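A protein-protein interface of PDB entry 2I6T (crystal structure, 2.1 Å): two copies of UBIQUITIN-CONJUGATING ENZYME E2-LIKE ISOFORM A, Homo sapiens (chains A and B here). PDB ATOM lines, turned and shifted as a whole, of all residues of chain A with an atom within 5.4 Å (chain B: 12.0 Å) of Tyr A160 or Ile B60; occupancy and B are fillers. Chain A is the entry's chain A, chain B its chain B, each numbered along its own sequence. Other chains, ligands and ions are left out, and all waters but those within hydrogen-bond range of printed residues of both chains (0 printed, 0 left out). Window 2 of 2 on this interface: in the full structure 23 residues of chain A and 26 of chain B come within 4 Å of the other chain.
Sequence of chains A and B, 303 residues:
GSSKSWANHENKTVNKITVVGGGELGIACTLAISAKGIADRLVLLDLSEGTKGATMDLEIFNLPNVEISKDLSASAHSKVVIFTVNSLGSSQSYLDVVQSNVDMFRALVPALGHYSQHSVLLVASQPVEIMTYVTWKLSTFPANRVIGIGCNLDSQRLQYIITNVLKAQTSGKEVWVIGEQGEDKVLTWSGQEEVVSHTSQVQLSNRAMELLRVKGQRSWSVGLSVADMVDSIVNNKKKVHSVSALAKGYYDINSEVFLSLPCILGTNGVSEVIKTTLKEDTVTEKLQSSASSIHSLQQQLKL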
ATOM      1  N   SER A 155      19.581 -18.180 -20.036  1.00  0.00           N
ATOM      2  CA  SER A 155      20.012 -19.234 -19.086  1.00  0.00           C
ATOM      3  C   SER A 155      19.320 -20.547 -19.352  1.00  0.00           C
ATOM      4  O   SER A 155      19.985 -21.579 -19.349  1.00  0.00           O
ATOM      5  CB  SER A 155      19.812 -18.824 -17.612  1.00  0.00           C
ATOM      6  OG  SER A 155      20.479 -17.589 -17.351  1.00  0.00           O
ATOM      7  N   GLN A 156      18.000 -20.524 -19.587  1.00  0.00           N
ATOM      8  CA  GLN A 156      17.256 -21.772 -19.824  1.00  0.00           C
ATOM      9  C   GLN A 156      17.663 -22.465 -21.103  1.00  0.00           C
ATOM     10  O   GLN A 156      17.710 -23.696 -21.155  1.00  0.00           O
ATOM     11  CB  GLN A 156      15.737 -21.562 -19.829  1.00  0.00           C
ATOM     12  CG  GLN A 156      15.136 -21.137 -18.440  1.00  0.00           C
ATOM     13  CD  GLN A 156      14.866 -22.313 -17.482  1.00  0.00           C
ATOM     14  OE1 GLN A 156      15.328 -23.451 -17.695  1.00  0.00           O
ATOM     15  NE2 GLN A 156      14.102 -22.038 -16.423  1.00  0.00           N
ATOM     16  N   ARG A 157      17.932 -21.672 -22.133  1.00  0.00           N
ATOM     17  CA  ARG A 157      18.375 -22.193 -23.419  1.00  0.00           C
ATOM     18  C   ARG A 157      19.721 -22.875 -23.228  1.00  0.00           C
ATOM     19  O   ARG A 157      19.945 -24.006 -23.674  1.00  0.00           O
ATOM     20  CB  ARG A 157      18.588 -21.026 -24.415  1.00  0.00           C
ATOM     21  CG  ARG A 157      17.330 -20.385 -24.981  1.00  0.00           C
ATOM     22  CD  ARG A 157      17.685 -19.029 -25.698  1.00  0.00           C
ATOM     23  NE  ARG A 157      16.550 -18.577 -26.490  1.00  0.00           N
ATOM     24  CZ  ARG A 157      16.439 -17.389 -27.070  1.00  0.00           C
ATOM     25  NH1 ARG A 157      17.406 -16.480 -26.958  1.00  0.00           N
ATOM     26  NH2 ARG A 157      15.344 -17.111 -27.776  1.00  0.00           N
ATOM     27  N   LEU A 158      20.625 -22.143 -22.582  1.00  0.00           N
ATOM     28  CA  LEU A 158      21.976 -22.627 -22.292  1.00  0.00           C
ATOM     29  C   LEU A 158      21.946 -23.930 -21.483  1.00  0.00           C
ATOM     30  O   LEU A 158      22.571 -24.920 -21.879  1.00  0.00           O
ATOM     31  CB  LEU A 158      22.768 -21.519 -21.582  1.00  0.00           C
ATOM     32  CG  LEU A 158      24.248 -21.717 -21.239  1.00  0.00           C
ATOM     33  CD1 LEU A 158      25.075 -21.938 -22.510  1.00  0.00           C
ATOM     34  CD2 LEU A 158      24.783 -20.531 -20.462  1.00  0.00           C
ATOM     35  N   GLN A 159      21.188 -23.958 -20.389  1.00  0.00           N
ATOM     36  CA  GLN A 159      21.080 -25.198 -19.579  1.00  0.00           C
ATOM     37  C   GLN A 159      20.456 -26.368 -20.353  1.00  0.00           C
ATOM     38  O   GLN A 159      20.944 -27.525 -20.298  1.00  0.00           O
ATOM     39  CB  GLN A 159      20.296 -24.918 -18.306  1.00  0.00           C
ATOM     40  CG  GLN A 159      21.006 -23.857 -17.452  1.00  0.00           C
ATOM     41  CD  GLN A 159      20.546 -23.875 -16.023  1.00  0.00           C
ATOM     42  OE1 GLN A 159      19.468 -24.396 -15.732  1.00  0.00           O
ATOM     43  NE2 GLN A 159      21.365 -23.318 -15.106  1.00  0.00           N
ATOM     44  N   TYR A 160      19.419 -26.041 -21.128  1.00  0.00           N
ATOM     45  CA  TYR A 160      18.777 -27.010 -21.981  1.00  0.00           C
ATOM     46  C   TYR A 160      19.749 -27.653 -22.957  1.00  0.00           C
ATOM     47  O   TYR A 160      19.810 -28.878 -23.081  1.00  0.00           O
ATOM     48  CB  TYR A 160      17.642 -26.374 -22.797  1.00  0.00           C
ATOM     49  CG  TYR A 160      16.961 -27.415 -23.666  1.00  0.00           C
ATOM     50  CD1 TYR A 160      15.943 -28.203 -23.156  1.00  0.00           C
ATOM     51  CD2 TYR A 160      17.361 -27.623 -24.986  1.00  0.00           C
ATOM     52  CE1 TYR A 160      15.324 -29.156 -23.931  1.00  0.00           C
ATOM     53  CE2 TYR A 160      16.750 -28.586 -25.779  1.00  0.00           C
ATOM     54  CZ  TYR A 160      15.727 -29.342 -25.236  1.00  0.00           C
ATOM     55  OH  TYR A 160      15.101 -30.303 -25.998  1.00  0.00           O
ATOM     56  N   ILE A 161      20.463 -26.811 -23.690  1.00  0.00           N
ATOM     57  CA  ILE A 161      21.406 -27.285 -24.673  1.00  0.00           C
ATOM     58  C   ILE A 161      22.431 -28.211 -24.029  1.00  0.00           C
ATOM     59  O   ILE A 161      22.683 -29.299 -24.524  1.00  0.00           O
ATOM     60  CB  ILE A 161      22.130 -26.115 -25.363  1.00  0.00           C
ATOM     61  CG1 ILE A 161      21.122 -25.327 -26.221  1.00  0.00           C
ATOM     62  CG2 ILE A 161      23.254 -26.663 -26.207  1.00  0.00           C
ATOM     63  CD1 ILE A 161      21.624 -23.901 -26.690  1.00  0.00           C
ATOM     64  N   ILE A 162      23.003 -27.777 -22.910  1.00  0.00           N
ATOM     65  CA  ILE A 162      23.996 -28.581 -22.220  1.00  0.00           C
ATOM     66  C   ILE A 162      23.386 -29.881 -21.677  1.00  0.00           C
ATOM     67  O   ILE A 162      23.970 -30.924 -21.871  1.00  0.00           O
ATOM     68  CB  ILE A 162      24.735 -27.777 -21.136  1.00  0.00           C
ATOM     69  CG1 ILE A 162      25.542 -26.623 -21.812  1.00  0.00           C
ATOM     70  CG2 ILE A 162      25.706 -28.669 -20.418  1.00  0.00           C
ATOM     71  CD1 ILE A 162      26.108 -25.555 -20.836  1.00  0.00           C
ATOM     72  N   THR A 163      22.217 -29.821 -21.031  1.00  0.00           N
ATOM     73  CA  THR A 163      21.675 -31.026 -20.352  1.00  0.00           C
ATOM     74  C   THR A 163      21.107 -32.015 -21.390  1.00  0.00           C
ATOM     75  O   THR A 163      21.372 -33.209 -21.307  1.00  0.00           O
ATOM     76  CB  THR A 163      20.574 -30.694 -19.323  1.00  0.00           C
ATOM     77  OG1 THR A 163      19.508 -29.997 -19.986  1.00  0.00           O
ATOM     78  CG2 THR A 163      21.077 -29.804 -18.222  1.00  0.00           C
ATOM     79  N   ASN A 164      20.354 -31.501 -22.371  1.00  0.00           N
ATOM     80  CA  ASN A 164      19.581 -32.313 -23.338  1.00  0.00           C
ATOM     81  C   ASN A 164      20.235 -32.549 -24.686  1.00  0.00           C
ATOM     82  O   ASN A 164      20.002 -33.587 -25.299  1.00  0.00           O
ATOM     83  CB  ASN A 164      18.216 -31.677 -23.613  1.00  0.00           C
ATOM     84  CG  ASN A 164      17.305 -31.709 -22.407  1.00  0.00           C
ATOM     85  OD1 ASN A 164      17.503 -30.989 -21.424  1.00  0.00           O
ATOM     86  ND2 ASN A 164      16.283 -32.532 -22.485  1.00  0.00           N
ATOM     87  N   VAL A 165      20.990 -31.571 -25.189  1.00  0.00           N
ATOM     88  CA  VAL A 165      21.698 -31.787 -26.441  1.00  0.00           C
ATOM     89  C   VAL A 165      23.097 -32.356 -26.184  1.00  0.00           C
ATOM     90  O   VAL A 165      23.472 -33.353 -26.777  1.00  0.00           O
ATOM     91  CB  VAL A 165      21.741 -30.527 -27.321  1.00  0.00           C
ATOM     92  CG1 VAL A 165      22.497 -30.807 -28.651  1.00  0.00           C
ATOM     93  CG2 VAL A 165      20.325 -30.056 -27.592  1.00  0.00           C
ATOM     94  N   LYS A 215      20.115 -16.424 -31.999  1.00  0.00           N
ATOM     95  CA  LYS A 215      18.950 -16.538 -31.115  1.00  0.00           C
ATOM     96  C   LYS A 215      18.659 -15.237 -30.372  1.00  0.00           C
ATOM     97  O   LYS A 215      19.536 -14.696 -29.683  1.00  0.00           O
ATOM     98  CB  LYS A 215      19.164 -17.663 -30.106  1.00  0.00           C
ATOM     99  CG  LYS A 215      18.835 -19.044 -30.606  1.00  0.00           C
ATOM    100  CD  LYS A 215      18.763 -20.002 -29.425  1.00  0.00           C
ATOM    101  CE  LYS A 215      18.458 -21.428 -29.854  1.00  0.00           C
ATOM    102  NZ  LYS A 215      17.969 -22.230 -28.699  1.00  0.00           N
ATOM    103  N   ILE B  27       4.682 -19.841 -35.137  1.00  0.00           N
ATOM    104  CA  ILE B  27       4.643 -19.903 -33.663  1.00  0.00           C
ATOM    105  C   ILE B  27       3.281 -19.443 -33.136  1.00  0.00           C
ATOM    106  O   ILE B  27       2.689 -20.111 -32.272  1.00  0.00           O
ATOM    107  CB  ILE B  27       5.842 -19.134 -32.972  1.00  0.00           C
ATOM    108  CG1 ILE B  27       7.141 -19.909 -33.158  1.00  0.00           C
ATOM    109  CG2 ILE B  27       5.619 -18.944 -31.465  1.00  0.00           C
ATOM    110  CD1 ILE B  27       8.018 -19.311 -34.213  1.00  0.00           C
ATOM    111  N   THR B  30       0.877 -22.153 -33.531  1.00  0.00           N
ATOM    112  CA  THR B  30       1.207 -23.207 -32.592  1.00  0.00           C
ATOM    113  C   THR B  30       0.799 -22.870 -31.165  1.00  0.00           C
ATOM    114  O   THR B  30       0.199 -23.703 -30.470  1.00  0.00           O
ATOM    115  CB  THR B  30       2.727 -23.505 -32.671  1.00  0.00           C
ATOM    116  OG1 THR B  30       3.060 -23.839 -34.021  1.00  0.00           O
ATOM    117  CG2 THR B  30       3.128 -24.653 -31.739  1.00  0.00           C
ATOM    118  N   LEU B  31       1.130 -21.665 -30.703  1.00  0.00           N
ATOM    119  CA  LEU B  31       0.743 -21.264 -29.328  1.00  0.00           C
ATOM    120  C   LEU B  31      -0.769 -21.231 -29.172  1.00  0.00           C
ATOM    121  O   LEU B  31      -1.302 -21.759 -28.179  1.00  0.00           O
ATOM    122  CB  LEU B  31       1.376 -19.924 -28.922  1.00  0.00           C
ATOM    123  CG  LEU B  31       2.806 -20.119 -28.376  1.00  0.00           C
ATOM    124  CD1 LEU B  31       3.542 -18.783 -28.218  1.00  0.00           C
ATOM    125  CD2 LEU B  31       2.730 -20.844 -27.063  1.00  0.00           C
ATOM    126  N   LEU B  42       1.256 -32.011 -32.047  1.00  0.00           N
ATOM    127  CA  LEU B  42       1.452 -30.884 -32.914  1.00  0.00           C
ATOM    128  C   LEU B  42       2.898 -30.840 -33.328  1.00  0.00           C
ATOM    129  O   LEU B  42       3.782 -30.727 -32.479  1.00  0.00           O
ATOM    130  CB  LEU B  42       1.050 -29.551 -32.248  1.00  0.00           C
ATOM    131  CG  LEU B  42       0.960 -28.355 -33.227  1.00  0.00           C
ATOM    132  CD1 LEU B  42       0.130 -27.255 -32.645  1.00  0.00           C
ATOM    133  CD2 LEU B  42       2.323 -27.807 -33.659  1.00  0.00           C
ATOM    134  N   LEU B  44       5.706 -28.773 -35.417  1.00  0.00           N
ATOM    135  CA  LEU B  44       6.093 -27.506 -36.022  1.00  0.00           C
ATOM    136  C   LEU B  44       7.351 -27.687 -36.874  1.00  0.00           C
ATOM    137  O   LEU B  44       8.415 -28.084 -36.356  1.00  0.00           O
ATOM    138  CB  LEU B  44       6.295 -26.419 -34.937  1.00  0.00           C
ATOM    139  CG  LEU B  44       6.814 -25.040 -35.357  1.00  0.00           C
ATOM    140  CD1 LEU B  44       5.992 -24.410 -36.481  1.00  0.00           C
ATOM    141  CD2 LEU B  44       6.808 -24.107 -34.177  1.00  0.00           C
ATOM    142  N   ASP B  46      10.379 -26.376 -38.721  1.00  0.00           N
ATOM    143  CA  ASP B  46      11.255 -25.226 -38.843  1.00  0.00           C
ATOM    144  C   ASP B  46      12.099 -25.429 -40.087  1.00  0.00           C
ATOM    145  O   ASP B  46      12.856 -26.372 -40.169  1.00  0.00           O
ATOM    146  CB  ASP B  46      12.112 -25.049 -37.577  1.00  0.00           C
ATOM    147  CG  ASP B  46      13.210 -23.986 -37.738  1.00  0.00           C
ATOM    148  OD1 ASP B  46      13.100 -23.109 -38.624  1.00  0.00           O
ATOM    149  OD2 ASP B  46      14.193 -24.050 -36.971  1.00  0.00           O
ATOM    150  N   GLY B  53      15.450 -21.452 -35.667  1.00  0.00           N
ATOM    151  CA  GLY B  53      16.416 -20.913 -34.709  1.00  0.00           C
ATOM    152  C   GLY B  53      15.821 -20.852 -33.311  1.00  0.00           C
ATOM    153  O   GLY B  53      15.956 -21.810 -32.531  1.00  0.00           O
ATOM    154  N   ALA B  54      15.148 -19.730 -33.013  1.00  0.00           N
ATOM    155  CA  ALA B  54      14.487 -19.494 -31.718  1.00  0.00           C
ATOM    156  C   ALA B  54      13.229 -20.349 -31.525  1.00  0.00           C
ATOM    157  O   ALA B  54      12.720 -20.472 -30.414  1.00  0.00           O
ATOM    158  CB  ALA B  54      14.168 -18.026 -31.556  1.00  0.00           C
ATOM    159  N   THR B  55      12.736 -20.929 -32.620  1.00  0.00           N
ATOM    160  CA  THR B  55      11.748 -22.016 -32.606  1.00  0.00           C
ATOM    161  C   THR B  55      12.008 -23.132 -31.567  1.00  0.00           C
ATOM    162  O   THR B  55      11.071 -23.738 -31.074  1.00  0.00           O
ATOM    163  CB  THR B  55      11.665 -22.639 -34.020  1.00  0.00           C
ATOM    164  OG1 THR B  55      11.433 -21.593 -34.977  1.00  0.00           O
ATOM    165  CG2 THR B  55      10.547 -23.641 -34.108  1.00  0.00           C
ATOM    166  N   MET B  56      13.269 -23.393 -31.226  1.00  0.00           N
ATOM    167  CA  MET B  56      13.603 -24.406 -30.215  1.00  0.00           C
ATOM    168  C   MET B  56      13.122 -24.013 -28.814  1.00  0.00           C
ATOM    169  O   MET B  56      12.911 -24.889 -27.955  1.00  0.00           O
ATOM    170  CB  MET B  56      15.110 -24.710 -30.199  1.00  0.00           C
ATOM    171  CG  MET B  56      15.500 -26.008 -29.439  1.00  0.00           C
ATOM    172  SD  MET B  56      17.263 -26.552 -29.424  1.00  0.00           S
ATOM    173  CE  MET B  56      18.099 -25.037 -28.942  1.00  0.00           C
ATOM    174  N   ASP B  57      12.936 -22.711 -28.579  1.00  0.00           N
ATOM    175  CA  ASP B  57      12.305 -22.251 -27.332  1.00  0.00           C
ATOM    176  C   ASP B  57      11.025 -23.017 -26.987  1.00  0.00           C
ATOM    177  O   ASP B  57      10.759 -23.284 -25.829  1.00  0.00           O
ATOM    178  CB  ASP B  57      12.030 -20.745 -27.362  1.00  0.00           C
ATOM    179  CG  ASP B  57      13.306 -19.922 -27.369  1.00  0.00           C
ATOM    180  OD1 ASP B  57      14.399 -20.455 -27.072  1.00  0.00           O
ATOM    181  OD2 ASP B  57      13.219 -18.729 -27.653  1.00  0.00           O
ATOM    182  N   LEU B  58      10.243 -23.388 -27.997  1.00  0.00           N
ATOM    183  CA  LEU B  58       8.994 -24.099 -27.759  1.00  0.00           C
ATOM    184  C   LEU B  58       9.256 -25.485 -27.151  1.00  0.00           C
ATOM    185  O   LEU B  58       8.486 -25.974 -26.328  1.00  0.00           O
ATOM    186  CB  LEU B  58       8.162 -24.171 -29.049  1.00  0.00           C
ATOM    187  CG  LEU B  58       7.281 -22.934 -29.321  1.00  0.00           C
ATOM    188  CD1 LEU B  58       8.085 -21.680 -29.729  1.00  0.00           C
ATOM    189  CD2 LEU B  58       6.234 -23.232 -30.381  1.00  0.00           C
ATOM    190  N   GLU B  59      10.353 -26.115 -27.557  1.00  0.00           N
ATOM    191  CA  GLU B  59      10.740 -27.386 -26.966  1.00  0.00           C
ATOM    192  C   GLU B  59      11.448 -27.160 -25.630  1.00  0.00           C
ATOM    193  O   GLU B  59      11.209 -27.875 -24.663  1.00  0.00           O
ATOM    194  CB  GLU B  59      11.643 -28.167 -27.919  1.00  0.00           C
ATOM    195  CG  GLU B  59      11.247 -29.634 -28.010  1.00  0.00           C
ATOM    196  CD  GLU B  59      11.749 -30.301 -29.279  1.00  0.00           C
ATOM    197  OE1 GLU B  59      12.968 -30.164 -29.566  1.00  0.00           O
ATOM    198  OE2 GLU B  59      10.927 -30.961 -29.974  1.00  0.00           O
ATOM    199  N   ILE B  60      12.312 -26.148 -25.597  1.00  0.00           N
ATOM    200  CA  ILE B  60      13.044 -25.772 -24.391  1.00  0.00           C
ATOM    201  C   ILE B  60      12.080 -25.498 -23.269  1.00  0.00           C
ATOM    202  O   ILE B  60      12.315 -25.901 -22.136  1.00  0.00           O
ATOM    203  CB  ILE B  60      13.948 -24.570 -24.644  1.00  0.00           C
ATOM    204  CG1 ILE B  60      15.169 -25.036 -25.414  1.00  0.00           C
ATOM    205  CG2 ILE B  60      14.385 -23.937 -23.353  1.00  0.00           C
ATOM    206  CD1 ILE B  60      15.991 -23.928 -26.070  1.00  0.00           C
ATOM    207  N   PHE B  61      10.963 -24.849 -23.580  1.00  0.00           N
ATOM    208  CA  PHE B  61      10.003 -24.544 -22.533  1.00  0.00           C
ATOM    209  C   PHE B  61       8.854 -25.538 -22.485  1.00  0.00           C
ATOM    210  O   PHE B  61       7.899 -25.344 -21.747  1.00  0.00           O
ATOM    211  CB  PHE B  61       9.566 -23.075 -22.591  1.00  0.00           C
ATOM    212  CG  PHE B  61      10.680 -22.103 -22.231  1.00  0.00           C
ATOM    213  CD1 PHE B  61      11.006 -21.859 -20.896  1.00  0.00           C
ATOM    214  CD2 PHE B  61      11.415 -21.469 -23.223  1.00  0.00           C
ATOM    215  CE1 PHE B  61      12.055 -20.990 -20.560  1.00  0.00           C
ATOM    216  CE2 PHE B  61      12.468 -20.587 -22.896  1.00  0.00           C
ATOM    217  CZ  PHE B  61      12.774 -20.332 -21.566  1.00  0.00           C
ATOM    218  N   ASN B  62       8.980 -26.612 -23.262  1.00  0.00           N
ATOM    219  CA  ASN B  62       8.220 -27.839 -23.037  1.00  0.00           C
ATOM    220  C   ASN B  62       6.721 -27.661 -23.231  1.00  0.00           C
ATOM    221  O   ASN B  62       5.915 -28.200 -22.470  1.00  0.00           O
ATOM    222  CB  ASN B  62       8.540 -28.361 -21.628  1.00  0.00           C
ATOM    223  CG  ASN B  62       8.312 -29.849 -21.470  1.00  0.00           C
ATOM    224  OD1 ASN B  62       8.773 -30.667 -22.278  1.00  0.00           O
ATOM    225  ND2 ASN B  62       7.616 -30.215 -20.395  1.00  0.00           N
ATOM    226  N   LEU B  63       6.352 -26.885 -24.249  1.00  0.00           N
ATOM    227  CA  LEU B  63       4.947 -26.738 -24.654  1.00  0.00           C
ATOM    228  C   LEU B  63       4.388 -28.121 -24.855  1.00  0.00           C
ATOM    229  O   LEU B  63       4.977 -28.904 -25.588  1.00  0.00           O
ATOM    230  CB  LEU B  63       4.852 -25.979 -25.964  1.00  0.00           C
ATOM    231  CG  LEU B  63       4.673 -24.478 -25.964  1.00  0.00           C
ATOM    232  CD1 LEU B  63       4.309 -24.107 -27.377  1.00  0.00           C
ATOM    233  CD2 LEU B  63       3.561 -24.080 -25.016  1.00  0.00           C
ATOM    234  N   PRO B  64       3.280 -28.452 -24.176  1.00  0.00           N
ATOM    235  CA  PRO B  64       2.927 -29.890 -24.175  1.00  0.00           C
ATOM    236  C   PRO B  64       2.521 -30.392 -25.567  1.00  0.00           C
ATOM    237  O   PRO B  64       1.829 -29.683 -26.309  1.00  0.00           O
ATOM    238  CB  PRO B  64       1.766 -29.995 -23.160  1.00  0.00           C
ATOM    239  CG  PRO B  64       1.713 -28.621 -22.447  1.00  0.00           C
ATOM    240  CD  PRO B  64       2.335 -27.621 -23.403  1.00  0.00           C
ATOM    241  N   ASN B  65       3.001 -31.595 -25.902  1.00  0.00           N
ATOM    242  CA  ASN B  65       2.825 -32.247 -27.223  1.00  0.00           C
ATOM    243  C   ASN B  65       3.317 -31.487 -28.461  1.00  0.00           C
ATOM    244  O   ASN B  65       2.912 -31.793 -29.580  1.00  0.00           O
ATOM    245  CB  ASN B  65       1.385 -32.720 -27.407  1.00  0.00           C
ATOM    246  CG  ASN B  65       0.912 -33.549 -26.240  1.00  0.00           C
ATOM    247  OD1 ASN B  65      -0.007 -33.156 -25.521  1.00  0.00           O
ATOM    248  ND2 ASN B  65       1.563 -34.692 -26.021  1.00  0.00           N
ATOM    249  N   VAL B  66       4.190 -30.508 -28.262  1.00  0.00           N
ATOM    250  CA  VAL B  66       4.797 -29.816 -29.395  1.00  0.00           C
ATOM    251  C   VAL B  66       6.113 -30.482 -29.760  1.00  0.00           C
ATOM    252  O   VAL B  66       7.014 -30.623 -28.934  1.00  0.00           O
ATOM    253  CB  VAL B  66       4.941 -28.309 -29.157  1.00  0.00           C
ATOM    254  CG1 VAL B  66       5.719 -27.623 -30.302  1.00  0.00           C
ATOM    255  CG2 VAL B  66       3.549 -27.699 -29.021  1.00  0.00           C
ATOM    256  N   GLU B  67       6.191 -30.930 -31.005  1.00  0.00           N
ATOM    257  CA  GLU B  67       7.417 -31.475 -31.549  1.00  0.00           C
ATOM    258  C   GLU B  67       7.920 -30.478 -32.564  1.00  0.00           C
ATOM    259  O   GLU B  67       7.187 -30.075 -33.472  1.00  0.00           O
ATOM    260  CB  GLU B  67       7.141 -32.836 -32.195  1.00  0.00           C
ATOM    261  CG  GLU B  67       8.381 -33.679 -32.492  1.00  0.00           C
ATOM    262  CD  GLU B  67       8.111 -34.811 -33.495  1.00  0.00           C
ATOM    263  OE1 GLU B  67       7.084 -35.532 -33.353  1.00  0.00           O
ATOM    264  OE2 GLU B  67       8.941 -34.979 -34.420  1.00  0.00           O
ATOM    265  N   ILE B  68       9.158 -30.040 -32.395  1.00  0.00           N
ATOM    266  CA  ILE B  68       9.798 -29.217 -33.400  1.00  0.00           C
ATOM    267  C   ILE B  68      10.677 -30.125 -34.261  1.00  0.00           C
ATOM    268  O   ILE B  68      11.352 -31.017 -33.740  1.00  0.00           O
ATOM    269  CB  ILE B  68      10.641 -28.090 -32.782  1.00  0.00           C
ATOM    270  CG1 ILE B  68       9.861 -27.293 -31.715  1.00  0.00           C
ATOM    271  CG2 ILE B  68      11.247 -27.208 -33.859  1.00  0.00           C
ATOM    272  CD1 ILE B  68       8.640 -26.515 -32.188  1.00  0.00           C
ATOM    273  N   SER B  69      10.662 -29.901 -35.575  1.00  0.00           N
ATOM    274  CA  SER B  69      11.457 -30.704 -36.490  1.00  0.00           C
ATOM    275  C   SER B  69      11.861 -29.941 -37.740  1.00  0.00           C
ATOM    276  O   SER B  69      11.231 -28.949 -38.120  1.00  0.00           O
ATOM    277  CB  SER B  69      10.725 -31.992 -36.876  1.00  0.00           C
ATOM    278  OG  SER B  69      11.526 -32.776 -37.756  1.00  0.00           O
ATOM    279  N   LYS B  70      12.920 -30.435 -38.371  1.00  0.00           N
ATOM    280  CA  LYS B  70      13.377 -29.958 -39.661  1.00  0.00           C
ATOM    281  C   LYS B  70      13.054 -31.019 -40.713  1.00  0.00           C
ATOM    282  O   LYS B  70      13.253 -30.814 -41.899  1.00  0.00           O
ATOM    283  CB  LYS B  70      14.888 -29.707 -39.599  1.00  0.00           C
ATOM    284  CG  LYS B  70      15.368 -28.565 -40.461  1.00  0.00           C
ATOM    285  CD  LYS B  70      15.502 -27.277 -39.650  1.00  0.00           C
ATOM    286  CE  LYS B  70      16.659 -27.313 -38.667  1.00  0.00           C
ATOM    287  NZ  LYS B  70      16.504 -26.200 -37.678  1.00  0.00           N
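The side-chain carboxylate (OD2) of Asp B57 is in salt-bridge range of the guanidinium group (NH2) of Arg A157 (2.7 Å).
The backbone carbonyl oxygen of Tyr A160 sits at hydrogen-bond distance from the side-chain hydroxyl of Thr A163 (3.3 Å).
OD2 of Asp B46 is in hydrogen-bond range of N of Gly B53 (3.2 Å).
Among the printed residues, pairs that only touch across the chains: Lys A215 with Met B56, Tyr A160 with Ile B60, Gln A156 with Phe B61, Lys A215 with Gly B53, Lys A215 with Ile B60, Arg A157 with Ile B60 and Gln A156 with Ile B60.
Of the printed residues of chain B, Gln A156 touches Ile B60 and Phe B61.
No residue of chain B comes within 4 Å of Leu A158.
Gln A159 touches none of the printed residues of chain B.
Tyr A160 touches just one residue of chain B: Ile B60 (3.4 Å).
Ile A161 touches none of the printed residues of chain B.
Thr A163 touches none of the printed residues of chain B.
No residue of chain B comes within 4 Å of Val A165.
Of the printed residues of chain B, Lys A215 touches Gly B53, Met B56 and Ile B60.
Of the printed residues of chain A, Gly B53 touches Lys A215.
Printed residues of chain A within 4 Å of Met B56: Lys A215 (2.8 Å).
Of the printed residues of chain A, Ile B60 touches Gln A156, Arg A157, Tyr A160 and Lys A215.
Of the printed residues of chain A, Phe B61 touches Gln A156.
The nearest printed residue of chain A that does not touch Ile B60 is Ile A161 (5.3 Å).
Of the 12 printed residues of chain A, 4 touch a printed residue of chain B.
Printed residues of chain A that touch a printed residue of chain B: Gln A156, Arg A157, Tyr A160 and Lys A215.
Along chain B the printed residues that touch a printed residue of chain A span positions 53 to 61.
No position is printed for both chains.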
